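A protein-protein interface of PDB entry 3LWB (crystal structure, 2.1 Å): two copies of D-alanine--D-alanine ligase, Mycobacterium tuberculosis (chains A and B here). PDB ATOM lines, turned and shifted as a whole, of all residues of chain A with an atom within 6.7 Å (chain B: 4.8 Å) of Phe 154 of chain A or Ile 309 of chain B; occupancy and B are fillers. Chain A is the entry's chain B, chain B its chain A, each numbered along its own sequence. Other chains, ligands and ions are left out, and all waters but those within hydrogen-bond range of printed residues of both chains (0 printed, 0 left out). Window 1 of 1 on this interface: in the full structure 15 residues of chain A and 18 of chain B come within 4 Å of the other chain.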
ATOM      1  N   LEU A 144      28.688   6.739  -6.821  1.00  0.00           N
ATOM      2  CA  LEU A 144      28.261   5.770  -5.827  1.00  0.00           C
ATOM      3  C   LEU A 144      26.831   6.006  -5.392  1.00  0.00           C
ATOM      4  O   LEU A 144      26.042   5.071  -5.287  1.00  0.00           O
ATOM      5  CB  LEU A 144      29.184   5.803  -4.611  1.00  0.00           C
ATOM      6  CG  LEU A 144      30.349   4.819  -4.660  1.00  0.00           C
ATOM      7  CD1 LEU A 144      31.258   5.016  -3.462  1.00  0.00           C
ATOM      8  CD2 LEU A 144      29.816   3.398  -4.701  1.00  0.00           C
ATOM      9  N   ALA A 147      24.462   4.917  -7.979  1.00  0.00           N
ATOM     10  CA  ALA A 147      24.355   3.469  -7.961  1.00  0.00           C
ATOM     11  C   ALA A 147      23.469   3.005  -6.817  1.00  0.00           C
ATOM     12  O   ALA A 147      22.636   2.122  -6.992  1.00  0.00           O
ATOM     13  CB  ALA A 147      25.725   2.836  -7.851  1.00  0.00           C
ATOM     14  N   VAL A 148      23.652   3.596  -5.642  1.00  0.00           N
ATOM     15  CA  VAL A 148      22.864   3.202  -4.483  1.00  0.00           C
ATOM     16  C   VAL A 148      21.368   3.440  -4.723  1.00  0.00           C
ATOM     17  O   VAL A 148      20.540   2.567  -4.467  1.00  0.00           O
ATOM     18  CB  VAL A 148      23.297   3.965  -3.221  1.00  0.00           C
ATOM     19  CG1 VAL A 148      22.407   3.589  -2.054  1.00  0.00           C
ATOM     20  CG2 VAL A 148      24.744   3.672  -2.899  1.00  0.00           C
ATOM     21  N   GLY A 149      21.029   4.625  -5.219  1.00  0.00           N
ATOM     22  CA  GLY A 149      19.639   4.978  -5.437  1.00  0.00           C
ATOM     23  C   GLY A 149      18.959   4.103  -6.474  1.00  0.00           C
ATOM     24  O   GLY A 149      17.739   3.988  -6.493  1.00  0.00           O
ATOM     25  N   ASP A 151      19.816   0.855  -6.784  1.00  0.00           N
ATOM     26  CA  ASP A 151      19.877  -0.513  -6.256  1.00  0.00           C
ATOM     27  C   ASP A 151      18.999  -0.648  -5.022  1.00  0.00           C
ATOM     28  O   ASP A 151      19.324  -0.116  -3.958  1.00  0.00           O
ATOM     29  CB  ASP A 151      21.329  -0.888  -5.918  1.00  0.00           C
ATOM     30  CG  ASP A 151      21.489  -2.348  -5.529  1.00  0.00           C
ATOM     31  OD1 ASP A 151      20.717  -2.847  -4.686  1.00  0.00           O
ATOM     32  OD2 ASP A 151      22.411  -2.995  -6.062  1.00  0.00           O
ATOM     33  N   LYS A 152      17.889  -1.364  -5.166  1.00  0.00           N
ATOM     34  CA  LYS A 152      16.922  -1.510  -4.086  1.00  0.00           C
ATOM     35  C   LYS A 152      17.542  -2.117  -2.824  1.00  0.00           C
ATOM     36  O   LYS A 152      17.160  -1.758  -1.712  1.00  0.00           O
ATOM     37  CB  LYS A 152      15.716  -2.347  -4.536  1.00  0.00           C
ATOM     38  CG  LYS A 152      14.848  -1.664  -5.584  1.00  0.00           C
ATOM     39  CD  LYS A 152      13.832  -2.624  -6.179  1.00  0.00           C
ATOM     40  CE  LYS A 152      13.225  -2.065  -7.468  1.00  0.00           C
ATOM     41  NZ  LYS A 152      14.171  -2.136  -8.615  1.00  0.00           N
ATOM     42  N   GLU A 153      18.486  -3.039  -2.995  1.00  0.00           N
ATOM     43  CA  GLU A 153      19.124  -3.655  -1.842  1.00  0.00           C
ATOM     44  C   GLU A 153      20.044  -2.671  -1.141  1.00  0.00           C
ATOM     45  O   GLU A 153      19.981  -2.512   0.068  1.00  0.00           O
ATOM     46  CB  GLU A 153      19.940  -4.887  -2.221  1.00  0.00           C
ATOM     47  CG  GLU A 153      20.727  -5.386  -1.022  1.00  0.00           C
ATOM     48  CD  GLU A 153      21.940  -6.177  -1.393  1.00  0.00           C
ATOM     49  OE1 GLU A 153      22.383  -6.091  -2.555  1.00  0.00           O
ATOM     50  OE2 GLU A 153      22.447  -6.894  -0.512  1.00  0.00           O
ATOM     51  N   PHE A 154      20.918  -2.032  -1.908  1.00  0.00           N
ATOM     52  CA  PHE A 154      21.818  -1.033  -1.347  1.00  0.00           C
ATOM     53  C   PHE A 154      21.049   0.090  -0.638  1.00  0.00           C
ATOM     54  O   PHE A 154      21.414   0.511   0.464  1.00  0.00           O
ATOM     55  CB  PHE A 154      22.749  -0.485  -2.428  1.00  0.00           C
ATOM     56  CG  PHE A 154      23.974  -1.329  -2.647  1.00  0.00           C
ATOM     57  CD1 PHE A 154      23.963  -2.681  -2.329  1.00  0.00           C
ATOM     58  CD2 PHE A 154      25.129  -0.780  -3.175  1.00  0.00           C
ATOM     59  CE1 PHE A 154      25.084  -3.474  -2.526  1.00  0.00           C
ATOM     60  CE2 PHE A 154      26.259  -1.568  -3.377  1.00  0.00           C
ATOM     61  CZ  PHE A 154      26.232  -2.918  -3.051  1.00  0.00           C
ATOM     62  N   THR A 155      19.979   0.558  -1.267  1.00  0.00           N
ATOM     63  CA  THR A 155      19.145   1.587  -0.671  1.00  0.00           C
ATOM     64  C   THR A 155      18.661   1.177   0.714  1.00  0.00           C
ATOM     65  O   THR A 155      18.856   1.910   1.675  1.00  0.00           O
ATOM     66  CB  THR A 155      17.952   1.955  -1.578  1.00  0.00           C
ATOM     67  OG1 THR A 155      18.413   2.786  -2.654  1.00  0.00           O
ATOM     68  CG2 THR A 155      16.881   2.705  -0.786  1.00  0.00           C
ATOM     69  N   LYS A 156      18.043   0.004   0.823  1.00  0.00           N
ATOM     70  CA  LYS A 156      17.496  -0.437   2.104  1.00  0.00           C
ATOM     71  C   LYS A 156      18.586  -0.702   3.139  1.00  0.00           C
ATOM     72  O   LYS A 156      18.406  -0.405   4.321  1.00  0.00           O
ATOM     73  CB  LYS A 156      16.604  -1.668   1.938  1.00  0.00           C
ATOM     74  CG  LYS A 156      15.418  -1.454   1.004  1.00  0.00           C
ATOM     75  CD  LYS A 156      14.370  -2.542   1.168  1.00  0.00           C
ATOM     76  CE  LYS A 156      13.528  -2.711  -0.093  1.00  0.00           C
ATOM     77  NZ  LYS A 156      12.800  -1.473  -0.486  1.00  0.00           N
ATOM     78  N   LYS A 157      19.709  -1.261   2.690  1.00  0.00           N
ATOM     79  CA  LYS A 157      20.862  -1.487   3.557  1.00  0.00           C
ATOM     80  C   LYS A 157      21.299  -0.199   4.225  1.00  0.00           C
ATOM     81  O   LYS A 157      21.269  -0.078   5.444  1.00  0.00           O
ATOM     82  CB  LYS A 157      22.055  -2.026   2.762  1.00  0.00           C
ATOM     83  CG  LYS A 157      22.022  -3.501   2.468  1.00  0.00           C
ATOM     84  CD  LYS A 157      23.026  -3.834   1.376  1.00  0.00           C
ATOM     85  CE  LYS A 157      24.331  -4.373   1.939  1.00  0.00           C
ATOM     86  NZ  LYS A 157      24.310  -5.853   1.976  1.00  0.00           N
ATOM     87  N   LEU A 158      21.728   0.751   3.406  1.00  0.00           N
ATOM     88  CA  LEU A 158      22.285   2.003   3.894  1.00  0.00           C
ATOM     89  C   LEU A 158      21.278   2.830   4.697  1.00  0.00           C
ATOM     90  O   LEU A 158      21.654   3.541   5.634  1.00  0.00           O
ATOM     91  CB  LEU A 158      22.847   2.813   2.728  1.00  0.00           C
ATOM     92  CG  LEU A 158      24.072   2.177   2.063  1.00  0.00           C
ATOM     93  CD1 LEU A 158      24.547   2.996   0.878  1.00  0.00           C
ATOM     94  CD2 LEU A 158      25.186   2.019   3.081  1.00  0.00           C
ATOM     95  N   LEU A 159      20.004   2.736   4.328  1.00  0.00           N
ATOM     96  CA  LEU A 159      18.946   3.426   5.059  1.00  0.00           C
ATOM     97  C   LEU A 159      18.767   2.827   6.448  1.00  0.00           C
ATOM     98  O   LEU A 159      18.720   3.548   7.439  1.00  0.00           O
ATOM     99  CB  LEU A 159      17.625   3.371   4.288  1.00  0.00           C
ATOM    100  CG  LEU A 159      17.282   4.593   3.439  1.00  0.00           C
ATOM    101  CD1 LEU A 159      18.540   5.225   2.885  1.00  0.00           C
ATOM    102  CD2 LEU A 159      16.301   4.235   2.315  1.00  0.00           C
ATOM    103  N   TYR A 169      12.958  -7.187   3.681  1.00  0.00           N
ATOM    104  CA  TYR A 169      13.343  -7.700   2.374  1.00  0.00           C
ATOM    105  C   TYR A 169      14.343  -8.837   2.516  1.00  0.00           C
ATOM    106  O   TYR A 169      14.874  -9.076   3.597  1.00  0.00           O
ATOM    107  CB  TYR A 169      13.963  -6.586   1.515  1.00  0.00           C
ATOM    108  CG  TYR A 169      15.341  -6.168   1.985  1.00  0.00           C
ATOM    109  CD1 TYR A 169      15.495  -5.327   3.080  1.00  0.00           C
ATOM    110  CD2 TYR A 169      16.485  -6.635   1.355  1.00  0.00           C
ATOM    111  CE1 TYR A 169      16.749  -4.955   3.534  1.00  0.00           C
ATOM    112  CE2 TYR A 169      17.749  -6.272   1.802  1.00  0.00           C
ATOM    113  CZ  TYR A 169      17.873  -5.429   2.892  1.00  0.00           C
ATOM    114  OH  TYR A 169      19.126  -5.056   3.339  1.00  0.00           O
ATOM    115  N   ARG A 173      20.826 -13.964  -4.882  1.00  0.00           N
ATOM    116  CA  ARG A 173      21.898 -13.942  -5.865  1.00  0.00           C
ATOM    117  C   ARG A 173      22.131 -15.357  -6.365  1.00  0.00           C
ATOM    118  O   ARG A 173      22.034 -16.308  -5.591  1.00  0.00           O
ATOM    119  CB  ARG A 173      23.180 -13.415  -5.226  1.00  0.00           C
ATOM    120  CG  ARG A 173      23.033 -12.048  -4.585  1.00  0.00           C
ATOM    121  CD  ARG A 173      24.256 -11.740  -3.754  1.00  0.00           C
ATOM    122  NE  ARG A 173      24.577 -10.317  -3.767  1.00  0.00           N
ATOM    123  CZ  ARG A 173      24.239  -9.476  -2.798  1.00  0.00           C
ATOM    124  NH1 ARG A 173      23.572  -9.931  -1.746  1.00  0.00           N
ATOM    125  NH2 ARG A 173      24.569  -8.190  -2.881  1.00  0.00           N
ATOM    126  N   LYS A 226      20.536 -10.271  -9.657  1.00  0.00           N
ATOM    127  CA  LYS A 226      20.185  -9.987  -8.272  1.00  0.00           C
ATOM    128  C   LYS A 226      18.698  -9.667  -8.157  1.00  0.00           C
ATOM    129  O   LYS A 226      18.208  -8.709  -8.760  1.00  0.00           O
ATOM    130  CB  LYS A 226      21.040  -8.844  -7.711  1.00  0.00           C
ATOM    131  CG  LYS A 226      20.894  -8.656  -6.207  1.00  0.00           C
ATOM    132  CD  LYS A 226      22.020  -7.806  -5.618  1.00  0.00           C
ATOM    133  CE  LYS A 226      21.849  -6.327  -5.916  1.00  0.00           C
ATOM    134  NZ  LYS A 226      22.806  -5.499  -5.108  1.00  0.00           N
ATOM    135  N   ILE A 228      15.368  -8.939  -5.605  1.00  0.00           N
ATOM    136  CA  ILE A 228      14.934  -8.591  -4.259  1.00  0.00           C
ATOM    137  C   ILE A 228      13.495  -9.027  -4.010  1.00  0.00           C
ATOM    138  O   ILE A 228      12.625  -8.855  -4.863  1.00  0.00           O
ATOM    139  CB  ILE A 228      15.107  -7.080  -3.954  1.00  0.00           C
ATOM    140  CG1 ILE A 228      14.981  -6.825  -2.444  1.00  0.00           C
ATOM    141  CG2 ILE A 228      14.094  -6.253  -4.706  1.00  0.00           C
ATOM    142  CD1 ILE A 228      15.249  -5.384  -2.046  1.00  0.00           C
ATOM    143  N   ILE A 309      22.946   8.002   1.875  1.00  0.00           N
ATOM    144  CA  ILE A 309      23.525   7.437   0.662  1.00  0.00           C
ATOM    145  C   ILE A 309      24.546   8.374   0.040  1.00  0.00           C
ATOM    146  O   ILE A 309      24.941   8.192  -1.108  1.00  0.00           O
ATOM    147  CB  ILE A 309      22.449   7.091  -0.386  1.00  0.00           C
ATOM    148  CG1 ILE A 309      21.794   8.365  -0.934  1.00  0.00           C
ATOM    149  CG2 ILE A 309      21.417   6.148   0.208  1.00  0.00           C
ATOM    150  CD1 ILE A 309      20.992   8.130  -2.217  1.00  0.00           C
ATOM    151  N   ALA B 145      32.102  -2.252  -7.300  1.00  0.00           N
ATOM    152  CA  ALA B 145      32.569  -2.913  -6.082  1.00  0.00           C
ATOM    153  C   ALA B 145      33.899  -2.318  -5.635  1.00  0.00           C
ATOM    154  O   ALA B 145      34.160  -2.163  -4.442  1.00  0.00           O
ATOM    155  CB  ALA B 145      32.689  -4.427  -6.291  1.00  0.00           C
ATOM    156  N   VAL B 148      33.344   1.100  -3.985  1.00  0.00           N
ATOM    157  CA  VAL B 148      32.881   0.805  -2.635  1.00  0.00           C
ATOM    158  C   VAL B 148      34.032   0.341  -1.756  1.00  0.00           C
ATOM    159  O   VAL B 148      34.279   0.912  -0.699  1.00  0.00           O
ATOM    160  CB  VAL B 148      31.806  -0.287  -2.640  1.00  0.00           C
ATOM    161  CG1 VAL B 148      31.577  -0.810  -1.233  1.00  0.00           C
ATOM    162  CG2 VAL B 148      30.519   0.253  -3.238  1.00  0.00           C
ATOM    163  N   THR B 155      32.273   0.907   2.822  1.00  0.00           N
ATOM    164  CA  THR B 155      32.546  -0.496   3.099  1.00  0.00           C
ATOM    165  C   THR B 155      32.018  -0.880   4.486  1.00  0.00           C
ATOM    166  O   THR B 155      31.252  -1.837   4.627  1.00  0.00           O
ATOM    167  CB  THR B 155      34.048  -0.828   2.976  1.00  0.00           C
ATOM    168  OG1 THR B 155      34.443  -0.748   1.600  1.00  0.00           O
ATOM    169  CG2 THR B 155      34.318  -2.226   3.473  1.00  0.00           C
ATOM    170  N   LEU B 158      28.149  -0.866   4.640  1.00  0.00           N
ATOM    171  CA  LEU B 158      27.519  -2.014   3.990  1.00  0.00           C
ATOM    172  C   LEU B 158      27.718  -3.305   4.786  1.00  0.00           C
ATOM    173  O   LEU B 158      26.778  -4.090   4.953  1.00  0.00           O
ATOM    174  CB  LEU B 158      28.040  -2.175   2.551  1.00  0.00           C
ATOM    175  CG  LEU B 158      27.587  -1.074   1.590  1.00  0.00           C
ATOM    176  CD1 LEU B 158      28.273  -1.178   0.229  1.00  0.00           C
ATOM    177  CD2 LEU B 158      26.070  -1.116   1.442  1.00  0.00           C
ATOM    178  N   ALA B 305      30.923 -11.045   3.624  1.00  0.00           N
ATOM    179  CA  ALA B 305      31.516  -9.748   3.320  1.00  0.00           C
ATOM    180  C   ALA B 305      31.549  -9.502   1.801  1.00  0.00           C
ATOM    181  O   ALA B 305      31.182  -8.423   1.325  1.00  0.00           O
ATOM    182  CB  ALA B 305      32.913  -9.642   3.905  1.00  0.00           C
ATOM    183  N   PHE B 306      31.994 -10.503   1.052  1.00  0.00           N
ATOM    184  CA  PHE B 306      32.004 -10.439  -0.415  1.00  0.00           C
ATOM    185  C   PHE B 306      30.617 -10.040  -0.935  1.00  0.00           C
ATOM    186  O   PHE B 306      30.481  -9.106  -1.718  1.00  0.00           O
ATOM    187  CB  PHE B 306      32.419 -11.808  -0.978  1.00  0.00           C
ATOM    188  CG  PHE B 306      32.619 -11.836  -2.475  1.00  0.00           C
ATOM    189  CD1 PHE B 306      33.889 -11.744  -3.015  1.00  0.00           C
ATOM    190  CD2 PHE B 306      31.542 -11.982  -3.335  1.00  0.00           C
ATOM    191  CE1 PHE B 306      34.084 -11.791  -4.398  1.00  0.00           C
ATOM    192  CE2 PHE B 306      31.726 -12.027  -4.716  1.00  0.00           C
ATOM    193  CZ  PHE B 306      32.999 -11.927  -5.247  1.00  0.00           C
ATOM    194  N   ALA B 307      29.585 -10.746  -0.475  1.00  0.00           N
ATOM    195  CA  ALA B 307      28.212 -10.468  -0.896  1.00  0.00           C
ATOM    196  C   ALA B 307      27.746  -9.090  -0.431  1.00  0.00           C
ATOM    197  O   ALA B 307      26.975  -8.423  -1.120  1.00  0.00           O
ATOM    198  CB  ALA B 307      27.265 -11.550  -0.366  1.00  0.00           C
ATOM    199  N   ALA B 308      28.229  -8.665   0.733  1.00  0.00           N
ATOM    200  CA  ALA B 308      27.767  -7.424   1.354  1.00  0.00           C
ATOM    201  C   ALA B 308      28.034  -6.195   0.500  1.00  0.00           C
ATOM    202  O   ALA B 308      27.249  -5.241   0.514  1.00  0.00           O
ATOM    203  CB  ALA B 308      28.390  -7.253   2.745  1.00  0.00           C
ATOM    204  N   ILE B 309      29.142  -6.213  -0.240  1.00  0.00           N
ATOM    205  CA  ILE B 309      29.496  -5.101  -1.106  1.00  0.00           C
ATOM    206  C   ILE B 309      29.195  -5.434  -2.558  1.00  0.00           C
ATOM    207  O   ILE B 309      29.605  -4.715  -3.463  1.00  0.00           O
ATOM    208  CB  ILE B 309      30.980  -4.709  -0.962  1.00  0.00           C
ATOM    209  CG1 ILE B 309      31.887  -5.816  -1.524  1.00  0.00           C
ATOM    210  CG2 ILE B 309      31.298  -4.400   0.508  1.00  0.00           C
ATOM    211  CD1 ILE B 309      33.390  -5.417  -1.642  1.00  0.00           C
ATOM    212  N   ASP B 310      28.482  -6.534  -2.769  1.00  0.00           N
ATOM    213  CA  ASP B 310      28.130  -6.982  -4.114  1.00  0.00           C
ATOM    214  C   ASP B 310      29.383  -7.193  -4.970  1.00  0.00           C
ATOM    215  O   ASP B 310      29.405  -6.882  -6.152  1.00  0.00           O
ATOM    216  CB  ASP B 310      27.169  -5.982  -4.777  1.00  0.00           C
ATOM    217  CG  ASP B 310      26.189  -6.655  -5.738  1.00  0.00           C
ATOM    218  OD1 ASP B 310      25.369  -5.948  -6.368  1.00  0.00           O
ATOM    219  OD2 ASP B 310      26.235  -7.899  -5.860  1.00  0.00           O
ATOM    220  N   CYS B 311      30.431  -7.737  -4.370  1.00  0.00           N
ATOM    221  CA  CYS B 311      31.671  -7.956  -5.103  1.00  0.00           C
ATOM    222  C   CYS B 311      31.481  -8.928  -6.271  1.00  0.00           C
ATOM    223  O   CYS B 311      30.501  -9.671  -6.327  1.00  0.00           O
ATOM    224  CB  CYS B 311      32.760  -8.480  -4.163  1.00  0.00           C
ATOM    225  SG  CYS B 311      34.445  -8.114  -4.734  1.00  0.00           S
ATOM    226  N   ILE B 331      38.060  -5.397   3.366  1.00  0.00           N
ATOM    227  CA  ILE B 331      37.825  -6.300   2.243  1.00  0.00           C
ATOM    228  C   ILE B 331      38.466  -5.667   1.025  1.00  0.00           C
ATOM    229  O   ILE B 331      38.140  -4.546   0.641  1.00  0.00           O
ATOM    230  CB  ILE B 331      36.334  -6.636   1.995  1.00  0.00           C
ATOM    231  CG1 ILE B 331      36.180  -7.413   0.678  1.00  0.00           C
ATOM    232  CG2 ILE B 331      35.491  -5.368   1.984  1.00  0.00           C
ATOM    233  CD1 ILE B 331      34.846  -8.166   0.533  1.00  0.00           C
ATOM    234  N   THR B 333      39.447  -5.664  -2.922  1.00  0.00           N
ATOM    235  CA  THR B 333      38.928  -6.149  -4.196  1.00  0.00           C
ATOM    236  C   THR B 333      39.984  -6.314  -5.278  1.00  0.00           C
ATOM    237  O   THR B 333      39.649  -6.660  -6.412  1.00  0.00           O
ATOM    238  CB  THR B 333      37.822  -5.211  -4.750  1.00  0.00           C
ATOM    239  OG1 THR B 333      38.402  -3.965  -5.148  1.00  0.00           O
ATOM    240  CG2 THR B 333      36.759  -4.952  -3.693  1.00  0.00           C
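CG2 of Val 148 of chain B touches CD2 of Leu 144 of chain A, at 3.5 Å.
Phe 154 of chain A touches Ile 309 of chain B (CZ to O, 3.8 Å).
CZ of Phe 154 of chain A touches CB of Asp 310 of chain B, at 3.6 Å.
Lys 157 of chain A touches Leu 158 of chain B (CE to CD2, 3.7 Å).
Leu 158 of chain A touches Leu 158 of chain B (CD2 to CD2, 3.6 Å).
Phe 154 of chain A touches just these residues of chain B: Ile 309 and Asp 310.
Of the printed residues of chain B, Lys 157 of chain A touches Leu 158 and Ala 308.
Of the printed residues of chain B, Leu 158 of chain A touches Leu 158 (3.6 Å).
Ile 309 of chain A touches none of the printed residues of chain B.
Ala 145 of chain B touches none of the printed residues of chain A.
Of the printed residues of chain A, Ala 308 of chain B touches Lys 157.
Ile 309 of chain B touches just one residue of chain A: Phe 154 (3.8 Å).
The nearest residue of chain A that does not touch Ile 309 of chain B is Lys 157 of chain A (5.3 Å).
The nearest printed residue of chain A that does not touch Ala 307 of chain B is Glu 153 of chain A (4.8 Å).
The side-chain carboxylate (OD2) of Asp 310 of chain B lies within salt-bridge range of the guanidinium group (NH2) of Arg 173 of chain A (3.4 Å).
NZ of Lys 157 of chain A lies within hydrogen-bond range of O of Ala 308 of chain B, 3.3 Å away.
The side-chain carboxylate (OD1) of Asp 310 of chain B is in salt-bridge range of the side-chain amino group (NZ) of Lys 226 of chain A (2.9 Å).
The backbone carbonyl oxygen of Ala 307 of chain B lies within hydrogen-bond range of the guanidinium group of Arg 173 of chain A (3.0 Å).
Leu 158 of chain B touches its own counterpart, Leu 158 of chain A.
4 positions are printed for both chains.
Of the 13 printed residues of chain B, 6 touch a printed residue of chain A.
Hydrophobic or aromatic side chains of chain B within 4 Å of the printed part of chain A: Val 148 and Leu 158.
Of the 18 printed residues of chain A, 6 touch a printed residue of chain B.
Hydrophobic or aromatic side chains of chain A that line the printed part of chain B: Leu 144, Phe 154 and Leu 158.
Among the printed residues, 9 pairs touch across the chains.
Among the printed residues, Asp or Glu carboxylates within 4 Å of a Lys or Arg side-chain nitrogen of the other chain: Arg 173 of chain A with Asp 310 of chain B (3.4 Å) and Lys 226 of chain A with Asp 310 of chain B (2.9 Å).
OD1 of Asp 151 of chain A is in hydrogen-bond range of N of Phe 154 of chain A, 2.9 Å away.
The side-chain amino group of Lys 226 of chain A is in salt-bridge range of the side-chain carboxylate of Asp 151 of chain A (2.7 Å).
The guanidinium group (NH2) of Arg 173 of chain A lies within salt-bridge range of the side-chain carboxylate (OE1) of Glu 153 of chain A (3.0 Å).
The backbone carbonyl oxygen of Val 148 of chain B lies within hydrogen-bond range of the side-chain hydroxyl of Thr 155 of chain B (2.8 Å).
The side-chain carboxylate (OE2) of Glu 153 of chain A lies within salt-bridge range of the side-chain amino group (NZ) of Lys 157 of chain A (3.3 Å).
The side-chain amino group of Lys 226 of chain A is in salt-bridge range of the side-chain carboxylate of Glu 153 of chain A (2.7 Å).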
